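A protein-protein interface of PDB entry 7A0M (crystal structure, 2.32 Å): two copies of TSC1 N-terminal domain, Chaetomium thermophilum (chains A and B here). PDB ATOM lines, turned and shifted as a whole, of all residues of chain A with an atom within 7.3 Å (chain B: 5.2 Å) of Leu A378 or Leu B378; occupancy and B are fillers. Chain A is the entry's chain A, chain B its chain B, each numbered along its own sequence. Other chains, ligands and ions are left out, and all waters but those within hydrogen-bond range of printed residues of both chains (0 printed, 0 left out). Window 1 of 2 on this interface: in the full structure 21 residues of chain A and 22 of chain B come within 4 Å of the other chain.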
ATOM      1  N   PHE A 327     -36.466  21.335  11.164  1.00  0.00           N
ATOM      2  CA  PHE A 327     -35.350  20.439  11.451  1.00  0.00           C
ATOM      3  C   PHE A 327     -34.687  20.801  12.774  1.00  0.00           C
ATOM      4  O   PHE A 327     -34.358  19.919  13.575  1.00  0.00           O
ATOM      5  CB  PHE A 327     -34.334  20.486  10.306  1.00  0.00           C
ATOM      6  CG  PHE A 327     -33.179  19.530  10.469  1.00  0.00           C
ATOM      7  CD1 PHE A 327     -32.090  19.856  11.267  1.00  0.00           C
ATOM      8  CD2 PHE A 327     -33.176  18.311   9.812  1.00  0.00           C
ATOM      9  CE1 PHE A 327     -31.031  18.980  11.414  1.00  0.00           C
ATOM     10  CE2 PHE A 327     -32.118  17.431   9.956  1.00  0.00           C
ATOM     11  CZ  PHE A 327     -31.044  17.767  10.756  1.00  0.00           C
ATOM     12  N   TYR A 331     -34.478  18.264  15.814  1.00  0.00           N
ATOM     13  CA  TYR A 331     -33.151  17.848  16.248  1.00  0.00           C
ATOM     14  C   TYR A 331     -32.835  18.354  17.649  1.00  0.00           C
ATOM     15  O   TYR A 331     -32.098  17.698  18.392  1.00  0.00           O
ATOM     16  CB  TYR A 331     -32.104  18.343  15.250  1.00  0.00           C
ATOM     17  CG  TYR A 331     -30.678  18.014  15.625  1.00  0.00           C
ATOM     18  CD1 TYR A 331     -30.170  16.734  15.446  1.00  0.00           C
ATOM     19  CD2 TYR A 331     -29.834  18.987  16.148  1.00  0.00           C
ATOM     20  CE1 TYR A 331     -28.865  16.429  15.783  1.00  0.00           C
ATOM     21  CE2 TYR A 331     -28.527  18.691  16.488  1.00  0.00           C
ATOM     22  CZ  TYR A 331     -28.049  17.410  16.303  1.00  0.00           C
ATOM     23  OH  TYR A 331     -26.749  17.108  16.639  1.00  0.00           O
ATOM     24  N   PRO A 335     -33.000  14.513  19.184  1.00  0.00           N
ATOM     25  CA  PRO A 335     -32.002  14.281  18.122  1.00  0.00           C
ATOM     26  C   PRO A 335     -31.748  12.815  17.820  1.00  0.00           C
ATOM     27  O   PRO A 335     -31.665  12.437  16.644  1.00  0.00           O
ATOM     28  CB  PRO A 335     -30.745  14.962  18.679  1.00  0.00           C
ATOM     29  CG  PRO A 335     -30.934  14.934  20.160  1.00  0.00           C
ATOM     30  CD  PRO A 335     -32.403  15.141  20.375  1.00  0.00           C
ATOM     31  N   VAL A 339     -32.381  11.430  14.033  1.00  0.00           N
ATOM     32  CA  VAL A 339     -31.369  10.912  13.117  1.00  0.00           C
ATOM     33  C   VAL A 339     -31.568   9.421  12.884  1.00  0.00           C
ATOM     34  O   VAL A 339     -31.178   8.893  11.835  1.00  0.00           O
ATOM     35  CB  VAL A 339     -29.951  11.222  13.635  1.00  0.00           C
ATOM     36  CG1 VAL A 339     -29.797  12.712  13.904  1.00  0.00           C
ATOM     37  CG2 VAL A 339     -29.641  10.411  14.886  1.00  0.00           C
ATOM     38  N   ILE A 342     -34.089   9.372  10.116  1.00  0.00           N
ATOM     39  CA  ILE A 342     -33.448   9.662   8.837  1.00  0.00           C
ATOM     40  C   ILE A 342     -32.638   8.463   8.368  1.00  0.00           C
ATOM     41  O   ILE A 342     -32.570   8.178   7.165  1.00  0.00           O
ATOM     42  CB  ILE A 342     -32.575  10.928   8.960  1.00  0.00           C
ATOM     43  CG1 ILE A 342     -33.441  12.139   9.315  1.00  0.00           C
ATOM     44  CG2 ILE A 342     -31.802  11.184   7.675  1.00  0.00           C
ATOM     45  CD1 ILE A 342     -32.651  13.406   9.570  1.00  0.00           C
ATOM     46  N   SER A 369     -31.275  15.843   3.632  1.00  0.00           N
ATOM     47  CA  SER A 369     -30.997  16.286   4.991  1.00  0.00           C
ATOM     48  C   SER A 369     -29.563  16.766   5.180  1.00  0.00           C
ATOM     49  O   SER A 369     -29.240  17.287   6.253  1.00  0.00           O
ATOM     50  CB  SER A 369     -31.288  15.158   5.985  1.00  0.00           C
ATOM     51  OG  SER A 369     -32.650  14.776   5.946  1.00  0.00           O
ATOM     52  N   GLU A 370     -28.703  16.599   4.170  1.00  0.00           N
ATOM     53  CA  GLU A 370     -27.297  16.970   4.315  1.00  0.00           C
ATOM     54  C   GLU A 370     -27.126  18.460   4.594  1.00  0.00           C
ATOM     55  O   GLU A 370     -26.333  18.846   5.460  1.00  0.00           O
ATOM     56  CB  GLU A 370     -26.517  16.566   3.064  1.00  0.00           C
ATOM     57  CG  GLU A 370     -26.036  15.126   3.085  1.00  0.00           C
ATOM     58  CD  GLU A 370     -25.016  14.873   4.179  1.00  0.00           C
ATOM     59  OE1 GLU A 370     -23.906  15.440   4.101  1.00  0.00           O
ATOM     60  OE2 GLU A 370     -25.326  14.113   5.121  1.00  0.00           O
ATOM     61  N   PHE A 372     -29.047  20.403   6.098  1.00  0.00           N
ATOM     62  CA  PHE A 372     -29.428  20.696   7.475  1.00  0.00           C
ATOM     63  C   PHE A 372     -28.436  20.110   8.471  1.00  0.00           C
ATOM     64  O   PHE A 372     -28.210  20.702   9.532  1.00  0.00           O
ATOM     65  CB  PHE A 372     -30.832  20.165   7.759  1.00  0.00           C
ATOM     66  CG  PHE A 372     -31.900  20.790   6.909  1.00  0.00           C
ATOM     67  CD1 PHE A 372     -31.918  22.157   6.691  1.00  0.00           C
ATOM     68  CD2 PHE A 372     -32.890  20.011   6.332  1.00  0.00           C
ATOM     69  CE1 PHE A 372     -32.898  22.735   5.911  1.00  0.00           C
ATOM     70  CE2 PHE A 372     -33.874  20.584   5.549  1.00  0.00           C
ATOM     71  CZ  PHE A 372     -33.880  21.948   5.341  1.00  0.00           C
ATOM     72  N   ARG A 373     -27.849  18.953   8.153  1.00  0.00           N
ATOM     73  CA  ARG A 373     -26.838  18.365   9.028  1.00  0.00           C
ATOM     74  C   ARG A 373     -25.639  19.292   9.184  1.00  0.00           C
ATOM     75  O   ARG A 373     -25.110  19.455  10.290  1.00  0.00           O
ATOM     76  CB  ARG A 373     -26.386  17.012   8.482  1.00  0.00           C
ATOM     77  CG  ARG A 373     -25.355  16.325   9.361  1.00  0.00           C
ATOM     78  CD  ARG A 373     -24.738  15.122   8.671  1.00  0.00           C
ATOM     79  NE  ARG A 373     -24.015  15.507   7.461  1.00  0.00           N
ATOM     80  CZ  ARG A 373     -22.809  16.071   7.457  1.00  0.00           C
ATOM     81  NH1 ARG A 373     -22.182  16.320   8.600  1.00  0.00           N
ATOM     82  NH2 ARG A 373     -22.227  16.387   6.309  1.00  0.00           N
ATOM     83  N   LYS A 374     -25.196  19.909   8.087  1.00  0.00           N
ATOM     84  CA  LYS A 374     -24.046  20.805   8.106  1.00  0.00           C
ATOM     85  C   LYS A 374     -24.334  22.130   8.797  1.00  0.00           C
ATOM     86  O   LYS A 374     -23.448  22.992   8.834  1.00  0.00           O
ATOM     87  CB  LYS A 374     -23.566  21.068   6.678  1.00  0.00           C
ATOM     88  CG  LYS A 374     -23.113  19.825   5.929  1.00  0.00           C
ATOM     89  CD  LYS A 374     -22.605  20.177   4.539  1.00  0.00           C
ATOM     90  CE  LYS A 374     -22.293  18.928   3.731  1.00  0.00           C
ATOM     91  NZ  LYS A 374     -21.905  19.258   2.332  1.00  0.00           N
ATOM     92  N   GLN A 375     -25.536  22.318   9.339  1.00  0.00           N
ATOM     93  CA  GLN A 375     -25.901  23.540  10.038  1.00  0.00           C
ATOM     94  C   GLN A 375     -26.009  23.358  11.544  1.00  0.00           C
ATOM     95  O   GLN A 375     -26.285  24.334  12.250  1.00  0.00           O
ATOM     96  CB  GLN A 375     -27.234  24.078   9.501  1.00  0.00           C
ATOM     97  CG  GLN A 375     -27.165  24.665   8.103  1.00  0.00           C
ATOM     98  CD  GLN A 375     -28.531  25.062   7.578  1.00  0.00           C
ATOM     99  OE1 GLN A 375     -29.357  25.604   8.313  1.00  0.00           O
ATOM    100  NE2 GLN A 375     -28.777  24.797   6.299  1.00  0.00           N
ATOM    101  N   HIS A 376     -25.796  22.149  12.058  1.00  0.00           N
ATOM    102  CA  HIS A 376     -26.060  21.853  13.458  1.00  0.00           C
ATOM    103  C   HIS A 376     -24.865  21.176  14.112  1.00  0.00           C
ATOM    104  O   HIS A 376     -24.244  20.283  13.530  1.00  0.00           O
ATOM    105  CB  HIS A 376     -27.306  20.973  13.606  1.00  0.00           C
ATOM    106  CG  HIS A 376     -28.583  21.687  13.289  1.00  0.00           C
ATOM    107  ND1 HIS A 376     -29.010  21.910  11.998  1.00  0.00           N
ATOM    108  CD2 HIS A 376     -29.517  22.241  14.096  1.00  0.00           C
ATOM    109  CE1 HIS A 376     -30.158  22.563  12.024  1.00  0.00           C
ATOM    110  NE2 HIS A 376     -30.487  22.777  13.284  1.00  0.00           N
ATOM    111  N   LEU A 377     -24.555  21.617  15.328  1.00  0.00           N
ATOM    112  CA  LEU A 377     -23.513  21.003  16.134  1.00  0.00           C
ATOM    113  C   LEU A 377     -23.958  19.628  16.625  1.00  0.00           C
ATOM    114  O   LEU A 377     -25.142  19.281  16.599  1.00  0.00           O
ATOM    115  CB  LEU A 377     -23.175  21.888  17.334  1.00  0.00           C
ATOM    116  CG  LEU A 377     -22.680  23.310  17.071  1.00  0.00           C
ATOM    117  CD1 LEU A 377     -22.825  24.156  18.325  1.00  0.00           C
ATOM    118  CD2 LEU A 377     -21.233  23.284  16.613  1.00  0.00           C
ATOM    119  N   LEU A 378     -22.983  18.836  17.072  1.00  0.00           N
ATOM    120  CA  LEU A 378     -23.298  17.574  17.727  1.00  0.00           C
ATOM    121  C   LEU A 378     -24.139  17.835  18.971  1.00  0.00           C
ATOM    122  O   LEU A 378     -23.815  18.704  19.786  1.00  0.00           O
ATOM    123  CB  LEU A 378     -22.014  16.829  18.092  1.00  0.00           C
ATOM    124  CG  LEU A 378     -22.199  15.470  18.772  1.00  0.00           C
ATOM    125  CD1 LEU A 378     -22.841  14.476  17.813  1.00  0.00           C
ATOM    126  CD2 LEU A 378     -20.874  14.937  19.296  1.00  0.00           C
ATOM    127  N   HIS A 379     -25.226  17.084  19.113  1.00  0.00           N
ATOM    128  CA  HIS A 379     -26.166  17.335  20.196  1.00  0.00           C
ATOM    129  C   HIS A 379     -25.664  16.708  21.497  1.00  0.00           C
ATOM    130  O   HIS A 379     -25.140  15.590  21.484  1.00  0.00           O
ATOM    131  CB  HIS A 379     -27.544  16.775  19.846  1.00  0.00           C
ATOM    132  CG  HIS A 379     -28.658  17.348  20.664  1.00  0.00           C
ATOM    133  ND1 HIS A 379     -28.851  17.026  21.991  1.00  0.00           N
ATOM    134  CD2 HIS A 379     -29.652  18.207  20.339  1.00  0.00           C
ATOM    135  CE1 HIS A 379     -29.908  17.673  22.450  1.00  0.00           C
ATOM    136  NE2 HIS A 379     -30.413  18.395  21.467  1.00  0.00           N
ATOM    137  N   PRO A 380     -25.809  17.405  22.627  1.00  0.00           N
ATOM    138  CA  PRO A 380     -25.381  16.825  23.912  1.00  0.00           C
ATOM    139  C   PRO A 380     -26.120  15.551  24.296  1.00  0.00           C
ATOM    140  O   PRO A 380     -25.602  14.785  25.119  1.00  0.00           O
ATOM    141  CB  PRO A 380     -25.646  17.956  24.917  1.00  0.00           C
ATOM    142  CG  PRO A 380     -26.618  18.867  24.235  1.00  0.00           C
ATOM    143  CD  PRO A 380     -26.282  18.792  22.779  1.00  0.00           C
ATOM    144  N   ASN A 381     -27.314  15.304  23.744  1.00  0.00           N
ATOM    145  CA  ASN A 381     -28.025  14.064  24.046  1.00  0.00           C
ATOM    146  C   ASN A 381     -27.203  12.845  23.660  1.00  0.00           C
ATOM    147  O   ASN A 381     -27.346  11.778  24.270  1.00  0.00           O
ATOM    148  CB  ASN A 381     -29.373  14.030  23.327  1.00  0.00           C
ATOM    149  CG  ASN A 381     -30.437  14.830  24.043  1.00  0.00           C
ATOM    150  OD1 ASN A 381     -30.136  15.722  24.836  1.00  0.00           O
ATOM    151  ND2 ASN A 381     -31.696  14.509  23.769  1.00  0.00           N
ATOM    152  N   PHE A 382     -26.343  12.980  22.651  1.00  0.00           N
ATOM    153  CA  PHE A 382     -25.502  11.880  22.203  1.00  0.00           C
ATOM    154  C   PHE A 382     -24.455  11.488  23.240  1.00  0.00           C
ATOM    155  O   PHE A 382     -23.847  10.421  23.104  1.00  0.00           O
ATOM    156  CB  PHE A 382     -24.836  12.240  20.872  1.00  0.00           C
ATOM    157  CG  PHE A 382     -25.792  12.267  19.707  1.00  0.00           C
ATOM    158  CD1 PHE A 382     -26.256  11.088  19.146  1.00  0.00           C
ATOM    159  CD2 PHE A 382     -26.232  13.471  19.181  1.00  0.00           C
ATOM    160  CE1 PHE A 382     -27.138  11.111  18.077  1.00  0.00           C
ATOM    161  CE2 PHE A 382     -27.114  13.499  18.116  1.00  0.00           C
ATOM    162  CZ  PHE A 382     -27.566  12.319  17.564  1.00  0.00           C
ATOM    163  N   TYR A 383     -24.230  12.315  24.262  1.00  0.00           N
ATOM    164  CA  TYR A 383     -23.358  11.970  25.375  1.00  0.00           C
ATOM    165  C   TYR A 383     -24.118  11.424  26.568  1.00  0.00           C
ATOM    166  O   TYR A 383     -23.493  11.065  27.566  1.00  0.00           O
ATOM    167  CB  TYR A 383     -22.625  13.215  25.887  1.00  0.00           C
ATOM    168  CG  TYR A 383     -21.567  13.839  25.019  1.00  0.00           C
ATOM    169  CD1 TYR A 383     -21.049  13.187  23.915  1.00  0.00           C
ATOM    170  CD2 TYR A 383     -21.090  15.109  25.311  1.00  0.00           C
ATOM    171  CE1 TYR A 383     -20.077  13.785  23.129  1.00  0.00           C
ATOM    172  CE2 TYR A 383     -20.127  15.708  24.537  1.00  0.00           C
ATOM    173  CZ  TYR A 383     -19.624  15.044  23.448  1.00  0.00           C
ATOM    174  OH  TYR A 383     -18.661  15.656  22.685  1.00  0.00           O
ATOM    175  N   LEU A 412     -27.540  25.306  18.851  1.00  0.00           N
ATOM    176  CA  LEU A 412     -27.007  24.238  18.018  1.00  0.00           C
ATOM    177  C   LEU A 412     -26.810  24.646  16.565  1.00  0.00           C
ATOM    178  O   LEU A 412     -26.151  23.913  15.822  1.00  0.00           O
ATOM    179  CB  LEU A 412     -27.929  23.015  18.074  1.00  0.00           C
ATOM    180  CG  LEU A 412     -28.150  22.372  19.442  1.00  0.00           C
ATOM    181  CD1 LEU A 412     -29.346  21.443  19.390  1.00  0.00           C
ATOM    182  CD2 LEU A 412     -26.905  21.617  19.880  1.00  0.00           C
ATOM    183  N   VAL A 414     -25.264  26.494  13.466  1.00  0.00           N
ATOM    184  CA  VAL A 414     -24.029  27.168  13.081  1.00  0.00           C
ATOM    185  C   VAL A 414     -24.305  28.097  11.906  1.00  0.00           C
ATOM    186  O   VAL A 414     -23.655  29.137  11.759  1.00  0.00           O
ATOM    187  CB  VAL A 414     -22.909  26.157  12.755  1.00  0.00           C
ATOM    188  CG1 VAL A 414     -22.773  25.143  13.877  1.00  0.00           C
ATOM    189  CG2 VAL A 414     -23.160  25.457  11.428  1.00  0.00           C
ATOM    190  N   TYR B 331     -13.546  11.480  16.414  1.00  0.00           N
ATOM    191  CA  TYR B 331     -14.927  11.748  16.035  1.00  0.00           C
ATOM    192  C   TYR B 331     -15.125  11.644  14.529  1.00  0.00           C
ATOM    193  O   TYR B 331     -16.212  11.270  14.072  1.00  0.00           O
ATOM    194  CB  TYR B 331     -15.340  13.130  16.540  1.00  0.00           C
ATOM    195  CG  TYR B 331     -16.736  13.555  16.148  1.00  0.00           C
ATOM    196  CD1 TYR B 331     -17.848  13.045  16.804  1.00  0.00           C
ATOM    197  CD2 TYR B 331     -16.940  14.478  15.131  1.00  0.00           C
ATOM    198  CE1 TYR B 331     -19.127  13.436  16.452  1.00  0.00           C
ATOM    199  CE2 TYR B 331     -18.213  14.874  14.772  1.00  0.00           C
ATOM    200  CZ  TYR B 331     -19.303  14.349  15.436  1.00  0.00           C
ATOM    201  OH  TYR B 331     -20.571  14.744  15.080  1.00  0.00           O
ATOM    202  N   VAL B 339     -18.835   8.769  20.806  1.00  0.00           N
ATOM    203  CA  VAL B 339     -19.813   9.396  21.690  1.00  0.00           C
ATOM    204  C   VAL B 339     -20.442   8.361  22.614  1.00  0.00           C
ATOM    205  O   VAL B 339     -20.899   8.699  23.712  1.00  0.00           O
ATOM    206  CB  VAL B 339     -20.878  10.155  20.877  1.00  0.00           C
ATOM    207  CG1 VAL B 339     -20.219  11.149  19.930  1.00  0.00           C
ATOM    208  CG2 VAL B 339     -21.772   9.187  20.111  1.00  0.00           C
ATOM    209  N   ARG B 373     -17.447  19.263  21.763  1.00  0.00           N
ATOM    210  CA  ARG B 373     -18.744  19.051  21.128  1.00  0.00           C
ATOM    211  C   ARG B 373     -19.201  20.303  20.394  1.00  0.00           C
ATOM    212  O   ARG B 373     -19.728  20.224  19.279  1.00  0.00           O
ATOM    213  CB  ARG B 373     -19.783  18.638  22.169  1.00  0.00           C
ATOM    214  CG  ARG B 373     -21.157  18.378  21.582  1.00  0.00           C
ATOM    215  CD  ARG B 373     -22.211  18.204  22.663  1.00  0.00           C
ATOM    216  NE  ARG B 373     -22.373  19.406  23.480  1.00  0.00           N
ATOM    217  CZ  ARG B 373     -23.035  20.493  23.094  1.00  0.00           C
ATOM    218  NH1 ARG B 373     -23.600  20.545  21.897  1.00  0.00           N
ATOM    219  NH2 ARG B 373     -23.131  21.536  23.908  1.00  0.00           N
ATOM    220  N   HIS B 376     -17.842  20.748  16.624  1.00  0.00           N
ATOM    221  CA  HIS B 376     -18.006  19.745  15.582  1.00  0.00           C
ATOM    222  C   HIS B 376     -19.458  19.633  15.145  1.00  0.00           C
ATOM    223  O   HIS B 376     -20.371  19.596  15.976  1.00  0.00           O
ATOM    224  CB  HIS B 376     -17.490  18.383  16.054  1.00  0.00           C
ATOM    225  CG  HIS B 376     -16.000  18.321  16.185  1.00  0.00           C
ATOM    226  ND1 HIS B 376     -15.324  18.846  17.265  1.00  0.00           N
ATOM    227  CD2 HIS B 376     -15.054  17.809  15.363  1.00  0.00           C
ATOM    228  CE1 HIS B 376     -14.027  18.653  17.107  1.00  0.00           C
ATOM    229  NE2 HIS B 376     -13.836  18.026  15.960  1.00  0.00           N
ATOM    230  N   LEU B 377     -19.655  19.569  13.830  1.00  0.00           N
ATOM    231  CA  LEU B 377     -20.969  19.360  13.245  1.00  0.00           C
ATOM    232  C   LEU B 377     -21.437  17.925  13.474  1.00  0.00           C
ATOM    233  O   LEU B 377     -20.654  17.033  13.815  1.00  0.00           O
ATOM    234  CB  LEU B 377     -20.939  19.658  11.746  1.00  0.00           C
ATOM    235  CG  LEU B 377     -20.510  21.064  11.323  1.00  0.00           C
ATOM    236  CD1 LEU B 377     -20.121  21.074   9.853  1.00  0.00           C
ATOM    237  CD2 LEU B 377     -21.617  22.068  11.596  1.00  0.00           C
ATOM    238  N   LEU B 378     -22.738  17.711  13.288  1.00  0.00           N
ATOM    239  CA  LEU B 378     -23.283  16.360  13.310  1.00  0.00           C
ATOM    240  C   LEU B 378     -22.636  15.512  12.220  1.00  0.00           C
ATOM    241  O   LEU B 378     -22.539  15.932  11.062  1.00  0.00           O
ATOM    242  CB  LEU B 378     -24.800  16.397  13.124  1.00  0.00           C
ATOM    243  CG  LEU B 378     -25.514  15.042  13.138  1.00  0.00           C
ATOM    244  CD1 LEU B 378     -25.420  14.392  14.512  1.00  0.00           C
ATOM    245  CD2 LEU B 378     -26.965  15.189  12.705  1.00  0.00           C
ATOM    246  N   HIS B 379     -22.194  14.316  12.596  1.00  0.00           N
ATOM    247  CA  HIS B 379     -21.466  13.446  11.683  1.00  0.00           C
ATOM    248  C   HIS B 379     -22.442  12.703  10.772  1.00  0.00           C
ATOM    249  O   HIS B 379     -23.507  12.274  11.225  1.00  0.00           O
ATOM    250  CB  HIS B 379     -20.618  12.445  12.466  1.00  0.00           C
ATOM    251  CG  HIS B 379     -19.528  11.811  11.661  1.00  0.00           C
ATOM    252  ND1 HIS B 379     -19.772  10.858  10.696  1.00  0.00           N
ATOM    253  CD2 HIS B 379     -18.184  11.978  11.692  1.00  0.00           C
ATOM    254  CE1 HIS B 379     -18.627  10.475  10.158  1.00  0.00           C
ATOM    255  NE2 HIS B 379     -17.649  11.139  10.746  1.00  0.00           N
ATOM    256  N   PRO B 380     -22.113  12.549   9.487  1.00  0.00           N
ATOM    257  CA  PRO B 380     -23.010  11.805   8.586  1.00  0.00           C
ATOM    258  C   PRO B 380     -23.229  10.357   8.996  1.00  0.00           C
ATOM    259  O   PRO B 380     -24.235   9.764   8.585  1.00  0.00           O
ATOM    260  CB  PRO B 380     -22.304  11.895   7.225  1.00  0.00           C
ATOM    261  CG  PRO B 380     -21.374  13.048   7.338  1.00  0.00           C
ATOM    262  CD  PRO B 380     -20.967  13.139   8.775  1.00  0.00           C
ATOM    263  N   PHE B 382     -24.233   9.278  11.709  1.00  0.00           N
ATOM    264  CA  PHE B 382     -25.459   9.196  12.491  1.00  0.00           C
ATOM    265  C   PHE B 382     -26.691   9.033  11.607  1.00  0.00           C
ATOM    266  O   PHE B 382     -27.757   8.679  12.122  1.00  0.00           O
ATOM    267  CB  PHE B 382     -25.592  10.424  13.395  1.00  0.00           C
ATOM    268  CG  PHE B 382     -24.601  10.450  14.533  1.00  0.00           C
ATOM    269  CD1 PHE B 382     -24.764   9.625  15.635  1.00  0.00           C
ATOM    270  CD2 PHE B 382     -23.505  11.298  14.499  1.00  0.00           C
ATOM    271  CE1 PHE B 382     -23.854   9.646  16.677  1.00  0.00           C
ATOM    272  CE2 PHE B 382     -22.593  11.321  15.539  1.00  0.00           C
ATOM    273  CZ  PHE B 382     -22.769  10.494  16.629  1.00  0.00           C
ATOM    274  N   TYR B 383     -26.567   9.272  10.300  1.00  0.00           N
ATOM    275  CA  TYR B 383     -27.619   8.993   9.332  1.00  0.00           C
ATOM    276  C   TYR B 383     -27.447   7.658   8.640  1.00  0.00           C
ATOM    277  O   TYR B 383     -28.290   7.296   7.816  1.00  0.00           O
ATOM    278  CB  TYR B 383     -27.591  10.014   8.189  1.00  0.00           C
ATOM    279  CG  TYR B 383     -28.031  11.430   8.432  1.00  0.00           C
ATOM    280  CD1 TYR B 383     -28.719  11.798   9.574  1.00  0.00           C
ATOM    281  CD2 TYR B 383     -27.757  12.410   7.487  1.00  0.00           C
ATOM    282  CE1 TYR B 383     -29.118  13.112   9.767  1.00  0.00           C
ATOM    283  CE2 TYR B 383     -28.149  13.710   7.672  1.00  0.00           C
ATOM    284  CZ  TYR B 383     -28.829  14.057   8.810  1.00  0.00           C
ATOM    285  OH  TYR B 383     -29.211  15.365   8.972  1.00  0.00           O
ATOM    286  N   LEU B 412     -15.859  18.783   9.437  1.00  0.00           N
ATOM    287  CA  LEU B 412     -16.736  18.720  10.596  1.00  0.00           C
ATOM    288  C   LEU B 412     -16.405  19.772  11.646  1.00  0.00           C
ATOM    289  O   LEU B 412     -17.203  19.978  12.566  1.00  0.00           O
ATOM    290  CB  LEU B 412     -16.657  17.328  11.230  1.00  0.00           C
ATOM    291  CG  LEU B 412     -17.060  16.169  10.317  1.00  0.00           C
ATOM    292  CD1 LEU B 412     -16.591  14.850  10.901  1.00  0.00           C
ATOM    293  CD2 LEU B 412     -18.565  16.157  10.094  1.00  0.00           C
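OH of Tyr B383 is in hydrogen-bond range of O of Ser A369.
The backbone carbonyl oxygen (O) of Leu B378 is in hydrogen-bond range of the guanidinium group (NH1) of Arg A373 (2.5 Å).
The backbone carbonyl oxygen (O) of His A376 is in hydrogen-bond range of the backbone NH (N) of Leu B378 (3.0 Å).
O of Leu A378 is in hydrogen-bond range of NH1 of Arg B373 (2.8 Å).
The backbone carbonyl oxygen of His B376 lies within hydrogen-bond range of the backbone NH of Leu A378.
The backbone carbonyl oxygen (O) of Val A339 sits close to the backbone carbonyl oxygen (O) of Phe B382 (3.4 Å).
The backbone carbonyl oxygen (O) of Val B339 sits close to the backbone carbonyl oxygen (O) of Phe A382.
The side-chain hydroxyl (OH) of Tyr A331 lies within hydrogen-bond range of the backbone carbonyl oxygen (O) of Leu A377, at 2.7 Å.
The side-chain carboxylate (OE1) of Glu A370 is in salt-bridge range of the guanidinium group (NH2) of Arg A373 (2.9 Å).
The backbone carbonyl oxygen (O) of Phe A372 is in hydrogen-bond range of a ring nitrogen (ND1) of His A376, at 2.9 Å.
The backbone NH (N) of Leu A377 is in hydrogen-bond range of the backbone carbonyl oxygen (O) of Leu A412.
N of Asn A381 sits at hydrogen-bond distance from ND1 of His A379 (2.9 Å).
The backbone NH of Leu B377 lies within hydrogen-bond range of the backbone carbonyl oxygen of Leu B412 (2.8 Å).
Among the printed residues, merely in contact across the chains: Phe A327 with Tyr B383 (3.5 Å), Tyr A331 with Leu B378 (3.7 Å), Val A339 with Leu B378 (3.9 Å), Ile A342 with Tyr B383 (3.6 Å), Glu A370 with Tyr B383 (3.8 Å), Arg A373 with His B379 (3.9 Å), Arg A373 with Pro B380 (3.3 Å), Arg A373 with Tyr B383 (3.3 Å), Arg A373 with Leu B412 (3.9 Å), Lys A374 with Leu B377 (3.4 Å), His A376 with Leu B377 (3.4 Å), Leu A377 with His B376 (3.4 Å), Leu A378 with Tyr B331 (3.6 Å), Leu A378 with Val B339 (3.9 Å), Leu A378 with Leu B378 (3.96 Å), Leu A378 with Phe B382 (3.9 Å), His A379 with Arg B373 (3.9 Å), Pro A380 with Arg B373 (3.3 Å), Phe A382 with Phe B382 (3.7 Å), Tyr A383 with Arg B373 (3.2 Å) and Val A414 with Leu B377 (3.7 Å).
Leu A378 touches just these residues of chain B: Tyr B331, Val B339, Arg B373, His B376, Leu B378 and Phe B382.
Of chain A, only Tyr A331, Val A339, Arg A373, His A376 and Leu A378 come within 4 Å of Leu B378.
Of the printed residues of chain B, Ser A369 touches Tyr B383 (3.3 Å).
Printed residues of chain A within 4 Å of Leu B377: Lys A374 (3.4 Å), His A376 (3.4 Å) and Val A414 (3.7 Å).
Printed residues of chain B within 4 Å of Ile A342: Tyr B383.
Printed residues of chain B within 4 Å of Pro A380: Arg B373.
The nearest residue of chain B that does not touch Leu A378 is Leu B377 (4.02 Å).
Of the 21 printed residues of chain A, 16 touch a printed residue of chain B.
Val A339 touches Leu B378, and with the chains exchanged Leu A378 touches Val B339.
Arg A373 touches Leu B378, and with the chains exchanged Leu A378 touches Arg B373.
His A376 touches Leu B377, and with the chains exchanged Leu A377 touches His B376.
Leu A378 touches Phe B382, but with the chains exchanged Phe A382 does not touch Leu B378 (4.1 Å).
11 positions are printed for both chains.
Of the 28 pairs that touch across the chains among the printed residues, 20 have their exchanged pair printed and touching as well.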
